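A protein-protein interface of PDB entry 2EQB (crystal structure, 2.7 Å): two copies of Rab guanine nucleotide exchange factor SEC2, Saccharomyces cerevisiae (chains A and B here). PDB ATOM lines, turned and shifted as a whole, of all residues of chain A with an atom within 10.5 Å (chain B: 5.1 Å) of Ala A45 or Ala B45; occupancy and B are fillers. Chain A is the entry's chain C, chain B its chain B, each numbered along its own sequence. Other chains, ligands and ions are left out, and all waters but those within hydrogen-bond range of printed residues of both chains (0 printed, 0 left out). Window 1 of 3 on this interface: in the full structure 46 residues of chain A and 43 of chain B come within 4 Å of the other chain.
Arg A42 touches its own counterpart, Arg B42.
Arg A42 touches Ala B45, but with the chains exchanged Ala A45 does not touch Arg B42 (5.1 Å).
Ala B45 touches its own counterpart, Ala A45.
Glu A48 touches Ala B49, but with the chains exchanged Ala A49 does not touch Glu B48 (5.4 Å).
9 positions are printed for both chains.
Of the 9 pairs that touch across the chains among the printed residues, 4 have their exchanged pair printed and touching as well.
Among the printed residues, merely in contact across the chains: Leu A41 with Arg B42, Arg A42 with Leu B41, Arg A42 with Arg B42, Arg A42 with Ala B45, Ala A45 with Glu B46, Ala A45 with Ala B49 and Glu A48 with Ala B49.
Of chain A, only Arg A42 (3.7 Å) and Ala A45 (3.3 Å) come within 4 Å of Ala B45.
Of the printed residues of chain A, Glu B46 touches Ala A45.
No residue of chain A comes within 4 Å of Glu B47.
Ala B49 touches just these residues of chain A: Ala A45 and Glu A48.
Of the printed residues of chain B, Glu A48 touches Ala B49 (3.9 Å).
Printed residues of chain B within 4 Å of Glu A38: Arg B42.
Printed residues of chain A within 4 Å of Arg B42: Glu A38, Leu A41 and Arg A42.
Printed residues of chain A within 4 Å of Leu B41: Arg A42.
Of the printed residues of chain B, Arg A42 touches Leu B41 (3.1 Å), Arg B42 (3.1 Å) and Ala B45 (3.7 Å).
The nearest residue of chain A that does not touch Ala B45 is Glu A46 (4.4 Å).
The side-chain carboxylate (OE2) of Glu A38 is in salt-bridge range of the guanidinium group (NH1) of Arg B42 (3.9 Å).
The backbone carbonyl oxygen of Ala A45 lies close to the backbone carbonyl oxygen of Ala B45, at 3.3 Å.
The guanidinium group (NE) of Arg B42 lies within salt-bridge range of the side-chain carboxylate (OE1) of Glu B46, at 3.6 Å.
The side-chain amide nitrogen (ND2) of Asn A39 lies close to the guanidinium group (NH2) of Arg A42, 3.3 Å away.
NH1 of Arg A42 lies within salt-bridge range of OE1 of Glu A46 (3.8 Å).
Of the 17 printed residues of chain A, 5 touch a printed residue of chain B.
Printed residues of chain A that touch a printed residue of chain B: Glu A38, Leu A41, Arg A42, Ala A45 and Glu A48.
Hydrophobic or aromatic side chains of chain A that line the printed part of chain B: Leu A41 and Ala A45.
Of the 9 printed residues of chain B, 5 touch a printed residue of chain A.
Printed residues of chain B that touch a printed residue of chain A: Leu B41, Arg B42, Ala B45, Glu B46 and Ala B49.
Hydrophobic or aromatic side chains of chain B that line the printed part of chain A: Leu B41, Ala B45 and Ala B49.
Among the printed residues, Asp or Glu carboxylates within 4 Å of a Lys or Arg side-chain nitrogen of the other chain: Glu A38 with Arg B42.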
ATOM      1  N   LYS A  37     -27.114 -10.135  15.350  1.00  0.00           N
ATOM      2  CA  LYS A  37     -27.510  -8.771  15.037  1.00  0.00           C
ATOM      3  C   LYS A  37     -26.789  -8.369  13.751  1.00  0.00           C
ATOM      4  O   LYS A  37     -27.433  -8.085  12.742  1.00  0.00           O
ATOM      5  CB  LYS A  37     -27.127  -7.833  16.192  1.00  0.00           C
ATOM      6  CG  LYS A  37     -27.995  -6.588  16.321  1.00  0.00           C
ATOM      7  CD  LYS A  37     -28.061  -6.080  17.765  1.00  0.00           C
ATOM      8  CE  LYS A  37     -26.719  -5.571  18.271  1.00  0.00           C
ATOM      9  NZ  LYS A  37     -26.812  -5.091  19.683  1.00  0.00           N
ATOM     10  N   GLU A  38     -25.459  -8.370  13.773  1.00  0.00           N
ATOM     11  CA  GLU A  38     -24.711  -7.999  12.582  1.00  0.00           C
ATOM     12  C   GLU A  38     -24.978  -8.891  11.381  1.00  0.00           C
ATOM     13  O   GLU A  38     -24.546  -8.584  10.273  1.00  0.00           O
ATOM     14  CB  GLU A  38     -23.205  -7.947  12.854  1.00  0.00           C
ATOM     15  CG  GLU A  38     -22.711  -6.505  12.889  1.00  0.00           C
ATOM     16  CD  GLU A  38     -21.319  -6.321  12.313  1.00  0.00           C
ATOM     17  OE1 GLU A  38     -20.901  -7.130  11.452  1.00  0.00           O
ATOM     18  OE2 GLU A  38     -20.652  -5.345  12.715  1.00  0.00           O
ATOM     19  N   ASN A  39     -25.679  -9.997  11.586  1.00  0.00           N
ATOM     20  CA  ASN A  39     -26.002 -10.877  10.470  1.00  0.00           C
ATOM     21  C   ASN A  39     -27.308 -10.381   9.869  1.00  0.00           C
ATOM     22  O   ASN A  39     -27.602 -10.647   8.705  1.00  0.00           O
ATOM     23  CB  ASN A  39     -26.143 -12.329  10.939  1.00  0.00           C
ATOM     24  CG  ASN A  39     -26.812 -13.212   9.907  1.00  0.00           C
ATOM     25  OD1 ASN A  39     -28.014 -13.080   9.651  1.00  0.00           O
ATOM     26  ND2 ASN A  39     -26.039 -14.117   9.301  1.00  0.00           N
ATOM     27  N   GLU A  40     -28.094  -9.659  10.665  1.00  0.00           N
ATOM     28  CA  GLU A  40     -29.353  -9.117  10.169  1.00  0.00           C
ATOM     29  C   GLU A  40     -29.059  -8.023   9.161  1.00  0.00           C
ATOM     30  O   GLU A  40     -29.755  -7.890   8.159  1.00  0.00           O
ATOM     31  CB  GLU A  40     -30.211  -8.574  11.310  1.00  0.00           C
ATOM     32  CG  GLU A  40     -31.140  -9.622  11.888  1.00  0.00           C
ATOM     33  CD  GLU A  40     -31.890 -10.383  10.804  1.00  0.00           C
ATOM     34  OE1 GLU A  40     -31.245 -11.159  10.058  1.00  0.00           O
ATOM     35  OE2 GLU A  40     -33.123 -10.194  10.695  1.00  0.00           O
ATOM     36  N   LEU A  41     -28.024  -7.238   9.436  1.00  0.00           N
ATOM     37  CA  LEU A  41     -27.610  -6.190   8.517  1.00  0.00           C
ATOM     38  C   LEU A  41     -27.139  -6.871   7.248  1.00  0.00           C
ATOM     39  O   LEU A  41     -27.771  -6.765   6.200  1.00  0.00           O
ATOM     40  CB  LEU A  41     -26.443  -5.397   9.084  1.00  0.00           C
ATOM     41  CG  LEU A  41     -26.655  -4.867  10.485  1.00  0.00           C
ATOM     42  CD1 LEU A  41     -25.652  -3.754  10.711  1.00  0.00           C
ATOM     43  CD2 LEU A  41     -28.091  -4.368  10.641  1.00  0.00           C
ATOM     44  N   ARG A  42     -26.014  -7.569   7.355  1.00  0.00           N
ATOM     45  CA  ARG A  42     -25.458  -8.273   6.217  1.00  0.00           C
ATOM     46  C   ARG A  42     -26.568  -9.011   5.467  1.00  0.00           C
ATOM     47  O   ARG A  42     -26.468  -9.224   4.262  1.00  0.00           O
ATOM     48  CB  ARG A  42     -24.391  -9.266   6.675  1.00  0.00           C
ATOM     49  CG  ARG A  42     -23.371  -9.615   5.590  1.00  0.00           C
ATOM     50  CD  ARG A  42     -22.722 -10.969   5.834  1.00  0.00           C
ATOM     51  NE  ARG A  42     -23.708 -11.961   6.255  1.00  0.00           N
ATOM     52  CZ  ARG A  42     -23.705 -13.232   5.873  1.00  0.00           C
ATOM     53  NH1 ARG A  42     -22.763 -13.668   5.051  1.00  0.00           N
ATOM     54  NH2 ARG A  42     -24.644 -14.063   6.314  1.00  0.00           N
ATOM     55  N   THR A  43     -27.633  -9.392   6.170  1.00  0.00           N
ATOM     56  CA  THR A  43     -28.732 -10.094   5.517  1.00  0.00           C
ATOM     57  C   THR A  43     -29.611  -9.158   4.700  1.00  0.00           C
ATOM     58  O   THR A  43     -30.215  -9.570   3.714  1.00  0.00           O
ATOM     59  CB  THR A  43     -29.610 -10.854   6.536  1.00  0.00           C
ATOM     60  OG1 THR A  43     -29.303 -12.251   6.460  1.00  0.00           O
ATOM     61  CG2 THR A  43     -31.100 -10.650   6.247  1.00  0.00           C
ATOM     62  N   LYS A  44     -29.687  -7.901   5.108  1.00  0.00           N
ATOM     63  CA  LYS A  44     -30.499  -6.934   4.383  1.00  0.00           C
ATOM     64  C   LYS A  44     -29.712  -6.442   3.159  1.00  0.00           C
ATOM     65  O   LYS A  44     -30.263  -6.334   2.065  1.00  0.00           O
ATOM     66  CB  LYS A  44     -30.863  -5.766   5.304  1.00  0.00           C
ATOM     67  CG  LYS A  44     -32.249  -5.172   5.065  1.00  0.00           C
ATOM     68  CD  LYS A  44     -32.519  -4.033   6.040  1.00  0.00           C
ATOM     69  CE  LYS A  44     -33.890  -3.415   5.829  1.00  0.00           C
ATOM     70  NZ  LYS A  44     -34.092  -2.216   6.695  1.00  0.00           N
ATOM     71  N   ALA A  45     -28.422  -6.165   3.340  1.00  0.00           N
ATOM     72  CA  ALA A  45     -27.572  -5.703   2.241  1.00  0.00           C
ATOM     73  C   ALA A  45     -27.417  -6.791   1.179  1.00  0.00           C
ATOM     74  O   ALA A  45     -26.639  -6.657   0.232  1.00  0.00           O
ATOM     75  CB  ALA A  45     -26.201  -5.284   2.765  1.00  0.00           C
ATOM     76  N   GLU A  46     -28.146  -7.882   1.366  1.00  0.00           N
ATOM     77  CA  GLU A  46     -28.143  -8.988   0.423  1.00  0.00           C
ATOM     78  C   GLU A  46     -29.574  -9.019  -0.100  1.00  0.00           C
ATOM     79  O   GLU A  46     -29.805  -9.098  -1.306  1.00  0.00           O
ATOM     80  CB  GLU A  46     -27.786 -10.314   1.123  1.00  0.00           C
ATOM     81  CG  GLU A  46     -26.301 -10.461   1.502  1.00  0.00           C
ATOM     82  CD  GLU A  46     -25.935 -11.854   2.046  1.00  0.00           C
ATOM     83  OE1 GLU A  46     -24.719 -12.153   2.104  1.00  0.00           O
ATOM     84  OE2 GLU A  46     -26.842 -12.643   2.420  1.00  0.00           O
ATOM     85  N   GLU A  47     -30.529  -8.946   0.826  1.00  0.00           N
ATOM     86  CA  GLU A  47     -31.955  -8.932   0.497  1.00  0.00           C
ATOM     87  C   GLU A  47     -32.172  -7.767  -0.462  1.00  0.00           C
ATOM     88  O   GLU A  47     -33.053  -7.793  -1.328  1.00  0.00           O
ATOM     89  CB  GLU A  47     -32.789  -8.698   1.763  1.00  0.00           C
ATOM     90  CG  GLU A  47     -32.896  -9.897   2.680  1.00  0.00           C
ATOM     91  CD  GLU A  47     -33.942 -10.889   2.212  1.00  0.00           C
ATOM     92  OE1 GLU A  47     -34.016 -11.155   0.990  1.00  0.00           O
ATOM     93  OE2 GLU A  47     -34.687 -11.409   3.071  1.00  0.00           O
ATOM     94  N   GLU A  48     -31.357  -6.735  -0.282  1.00  0.00           N
ATOM     95  CA  GLU A  48     -31.418  -5.546  -1.114  1.00  0.00           C
ATOM     96  C   GLU A  48     -30.875  -5.899  -2.491  1.00  0.00           C
ATOM     97  O   GLU A  48     -31.646  -6.186  -3.407  1.00  0.00           O
ATOM     98  CB  GLU A  48     -30.596  -4.424  -0.470  1.00  0.00           C
ATOM     99  CG  GLU A  48     -30.357  -3.202  -1.346  1.00  0.00           C
ATOM    100  CD  GLU A  48     -30.020  -1.972  -0.525  1.00  0.00           C
ATOM    101  OE1 GLU A  48     -29.416  -1.023  -1.073  1.00  0.00           O
ATOM    102  OE2 GLU A  48     -30.375  -1.953   0.673  1.00  0.00           O
ATOM    103  N   ALA A  49     -29.552  -5.887  -2.629  1.00  0.00           N
ATOM    104  CA  ALA A  49     -28.901  -6.217  -3.891  1.00  0.00           C
ATOM    105  C   ALA A  49     -29.689  -7.224  -4.738  1.00  0.00           C
ATOM    106  O   ALA A  49     -29.737  -7.103  -5.961  1.00  0.00           O
ATOM    107  CB  ALA A  49     -27.510  -6.743  -3.627  1.00  0.00           C
ATOM    108  N   ASP A  50     -30.301  -8.219  -4.101  1.00  0.00           N
ATOM    109  CA  ASP A  50     -31.091  -9.194  -4.846  1.00  0.00           C
ATOM    110  C   ASP A  50     -32.281  -8.505  -5.491  1.00  0.00           C
ATOM    111  O   ASP A  50     -32.416  -8.510  -6.715  1.00  0.00           O
ATOM    112  CB  ASP A  50     -31.591 -10.314  -3.929  1.00  0.00           C
ATOM    113  CG  ASP A  50     -30.559 -11.398  -3.728  1.00  0.00           C
ATOM    114  OD1 ASP A  50     -30.267 -12.121  -4.704  1.00  0.00           O
ATOM    115  OD2 ASP A  50     -30.035 -11.523  -2.602  1.00  0.00           O
ATOM    116  N   LYS A  51     -33.136  -7.903  -4.669  1.00  0.00           N
ATOM    117  CA  LYS A  51     -34.315  -7.213  -5.175  1.00  0.00           C
ATOM    118  C   LYS A  51     -33.941  -6.461  -6.435  1.00  0.00           C
ATOM    119  O   LYS A  51     -34.544  -6.662  -7.486  1.00  0.00           O
ATOM    120  CB  LYS A  51     -34.862  -6.206  -4.161  1.00  0.00           C
ATOM    121  CG  LYS A  51     -36.250  -5.696  -4.543  1.00  0.00           C
ATOM    122  CD  LYS A  51     -36.641  -4.401  -3.836  1.00  0.00           C
ATOM    123  CE  LYS A  51     -38.040  -3.977  -4.277  1.00  0.00           C
ATOM    124  NZ  LYS A  51     -38.394  -2.588  -3.875  1.00  0.00           N
ATOM    125  N   LEU A  52     -32.925  -5.610  -6.322  1.00  0.00           N
ATOM    126  CA  LEU A  52     -32.473  -4.803  -7.448  1.00  0.00           C
ATOM    127  C   LEU A  52     -32.273  -5.650  -8.690  1.00  0.00           C
ATOM    128  O   LEU A  52     -32.955  -5.468  -9.702  1.00  0.00           O
ATOM    129  CB  LEU A  52     -31.153  -4.077  -7.118  1.00  0.00           C
ATOM    130  CG  LEU A  52     -30.675  -3.061  -8.173  1.00  0.00           C
ATOM    131  CD1 LEU A  52     -31.774  -2.045  -8.315  1.00  0.00           C
ATOM    132  CD2 LEU A  52     -29.352  -2.352  -7.809  1.00  0.00           C
ATOM    133  N   ASN A  53     -31.343  -6.594  -8.600  1.00  0.00           N
ATOM    134  CA  ASN A  53     -31.022  -7.436  -9.739  1.00  0.00           C
ATOM    135  C   ASN A  53     -32.183  -8.252 -10.270  1.00  0.00           C
ATOM    136  O   ASN A  53     -32.203  -8.585 -11.454  1.00  0.00           O
ATOM    137  CB  ASN A  53     -29.821  -8.327  -9.412  1.00  0.00           C
ATOM    138  CG  ASN A  53     -28.602  -7.514  -8.976  1.00  0.00           C
ATOM    139  OD1 ASN A  53     -27.462  -7.941  -9.137  1.00  0.00           O
ATOM    140  ND2 ASN A  53     -28.849  -6.337  -8.410  1.00  0.00           N
ATOM    141  N   LEU B  41     -17.970  -9.078   6.404  1.00  0.00           N
ATOM    142  CA  LEU B  41     -18.947  -9.457   5.398  1.00  0.00           C
ATOM    143  C   LEU B  41     -19.984  -8.361   5.255  1.00  0.00           C
ATOM    144  O   LEU B  41     -20.140  -7.789   4.179  1.00  0.00           O
ATOM    145  CB  LEU B  41     -19.642 -10.753   5.785  1.00  0.00           C
ATOM    146  CG  LEU B  41     -18.800 -12.017   5.914  1.00  0.00           C
ATOM    147  CD1 LEU B  41     -19.661 -13.164   5.469  1.00  0.00           C
ATOM    148  CD2 LEU B  41     -17.561 -11.965   5.044  1.00  0.00           C
ATOM    149  N   ARG B  42     -20.700  -8.076   6.339  1.00  0.00           N
ATOM    150  CA  ARG B  42     -21.701  -7.021   6.305  1.00  0.00           C
ATOM    151  C   ARG B  42     -21.047  -5.775   5.709  1.00  0.00           C
ATOM    152  O   ARG B  42     -21.705  -4.960   5.066  1.00  0.00           O
ATOM    153  CB  ARG B  42     -22.213  -6.713   7.708  1.00  0.00           C
ATOM    154  CG  ARG B  42     -23.447  -5.829   7.720  1.00  0.00           C
ATOM    155  CD  ARG B  42     -23.415  -4.873   8.895  1.00  0.00           C
ATOM    156  NE  ARG B  42     -22.194  -4.071   8.905  1.00  0.00           N
ATOM    157  CZ  ARG B  42     -21.944  -3.098   9.776  1.00  0.00           C
ATOM    158  NH1 ARG B  42     -22.833  -2.801  10.713  1.00  0.00           N
ATOM    159  NH2 ARG B  42     -20.806  -2.419   9.706  1.00  0.00           N
ATOM    160  N   THR B  43     -19.745  -5.634   5.929  1.00  0.00           N
ATOM    161  CA  THR B  43     -19.001  -4.511   5.373  1.00  0.00           C
ATOM    162  C   THR B  43     -19.137  -4.589   3.851  1.00  0.00           C
ATOM    163  O   THR B  43     -19.799  -3.751   3.242  1.00  0.00           O
ATOM    164  CB  THR B  43     -17.502  -4.574   5.816  1.00  0.00           C
ATOM    165  OG1 THR B  43     -17.294  -3.649   6.888  1.00  0.00           O
ATOM    166  CG2 THR B  43     -16.546  -4.237   4.675  1.00  0.00           C
ATOM    167  N   LYS B  44     -18.541  -5.620   3.254  1.00  0.00           N
ATOM    168  CA  LYS B  44     -18.575  -5.836   1.811  1.00  0.00           C
ATOM    169  C   LYS B  44     -20.008  -5.838   1.275  1.00  0.00           C
ATOM    170  O   LYS B  44     -20.341  -5.058   0.387  1.00  0.00           O
ATOM    171  CB  LYS B  44     -17.886  -7.160   1.485  1.00  0.00           C
ATOM    172  CG  LYS B  44     -16.514  -7.322   2.136  1.00  0.00           C
ATOM    173  CD  LYS B  44     -15.381  -7.134   1.144  1.00  0.00           C
ATOM    174  CE  LYS B  44     -14.050  -7.550   1.752  1.00  0.00           C
ATOM    175  NZ  LYS B  44     -12.993  -7.674   0.704  1.00  0.00           N
ATOM    176  N   ALA B  45     -20.849  -6.715   1.818  1.00  0.00           N
ATOM    177  CA  ALA B  45     -22.255  -6.810   1.413  1.00  0.00           C
ATOM    178  C   ALA B  45     -22.925  -5.448   1.244  1.00  0.00           C
ATOM    179  O   ALA B  45     -23.628  -5.213   0.259  1.00  0.00           O
ATOM    180  CB  ALA B  45     -23.039  -7.630   2.429  1.00  0.00           C
ATOM    181  N   GLU B  46     -22.721  -4.562   2.217  1.00  0.00           N
ATOM    182  CA  GLU B  46     -23.310  -3.227   2.175  1.00  0.00           C
ATOM    183  C   GLU B  46     -22.662  -2.344   1.103  1.00  0.00           C
ATOM    184  O   GLU B  46     -23.330  -1.508   0.501  1.00  0.00           O
ATOM    185  CB  GLU B  46     -23.191  -2.545   3.541  1.00  0.00           C
ATOM    186  CG  GLU B  46     -24.017  -3.180   4.656  1.00  0.00           C
ATOM    187  CD  GLU B  46     -23.983  -2.352   5.934  1.00  0.00           C
ATOM    188  OE1 GLU B  46     -22.903  -1.766   6.207  1.00  0.00           O
ATOM    189  OE2 GLU B  46     -25.023  -2.299   6.654  1.00  0.00           O
ATOM    190  N   GLU B  47     -21.361  -2.518   0.878  1.00  0.00           N
ATOM    191  CA  GLU B  47     -20.652  -1.745  -0.143  1.00  0.00           C
ATOM    192  C   GLU B  47     -21.255  -2.099  -1.494  1.00  0.00           C
ATOM    193  O   GLU B  47     -21.670  -1.235  -2.261  1.00  0.00           O
ATOM    194  CB  GLU B  47     -19.170  -2.126  -0.197  1.00  0.00           C
ATOM    195  CG  GLU B  47     -18.298  -1.662   0.941  1.00  0.00           C
ATOM    196  CD  GLU B  47     -16.961  -2.387   0.941  1.00  0.00           C
ATOM    197  OE1 GLU B  47     -16.367  -2.546  -0.147  1.00  0.00           O
ATOM    198  OE2 GLU B  47     -16.505  -2.799   2.025  1.00  0.00           O
ATOM    199  N   GLU B  48     -21.275  -3.395  -1.772  1.00  0.00           N
ATOM    200  CA  GLU B  48     -21.787  -3.926  -3.022  1.00  0.00           C
ATOM    201  C   GLU B  48     -23.196  -3.427  -3.346  1.00  0.00           C
ATOM    202  O   GLU B  48     -23.426  -2.878  -4.421  1.00  0.00           O
ATOM    203  CB  GLU B  48     -21.760  -5.453  -2.961  1.00  0.00           C
ATOM    204  CG  GLU B  48     -21.508  -6.139  -4.287  1.00  0.00           C
ATOM    205  CD  GLU B  48     -20.187  -5.741  -4.902  1.00  0.00           C
ATOM    206  OE1 GLU B  48     -19.210  -5.563  -4.143  1.00  0.00           O
ATOM    207  OE2 GLU B  48     -20.124  -5.618  -6.143  1.00  0.00           O
ATOM    208  N   ALA B  49     -24.139  -3.617  -2.428  1.00  0.00           N
ATOM    209  CA  ALA B  49     -25.507  -3.161  -2.658  1.00  0.00           C
ATOM    210  C   ALA B  49     -25.479  -1.683  -3.038  1.00  0.00           C
ATOM    211  O   ALA B  49     -26.454  -1.141  -3.564  1.00  0.00           O
ATOM    212  CB  ALA B  49     -26.353  -3.367  -1.406  1.00  0.00           C
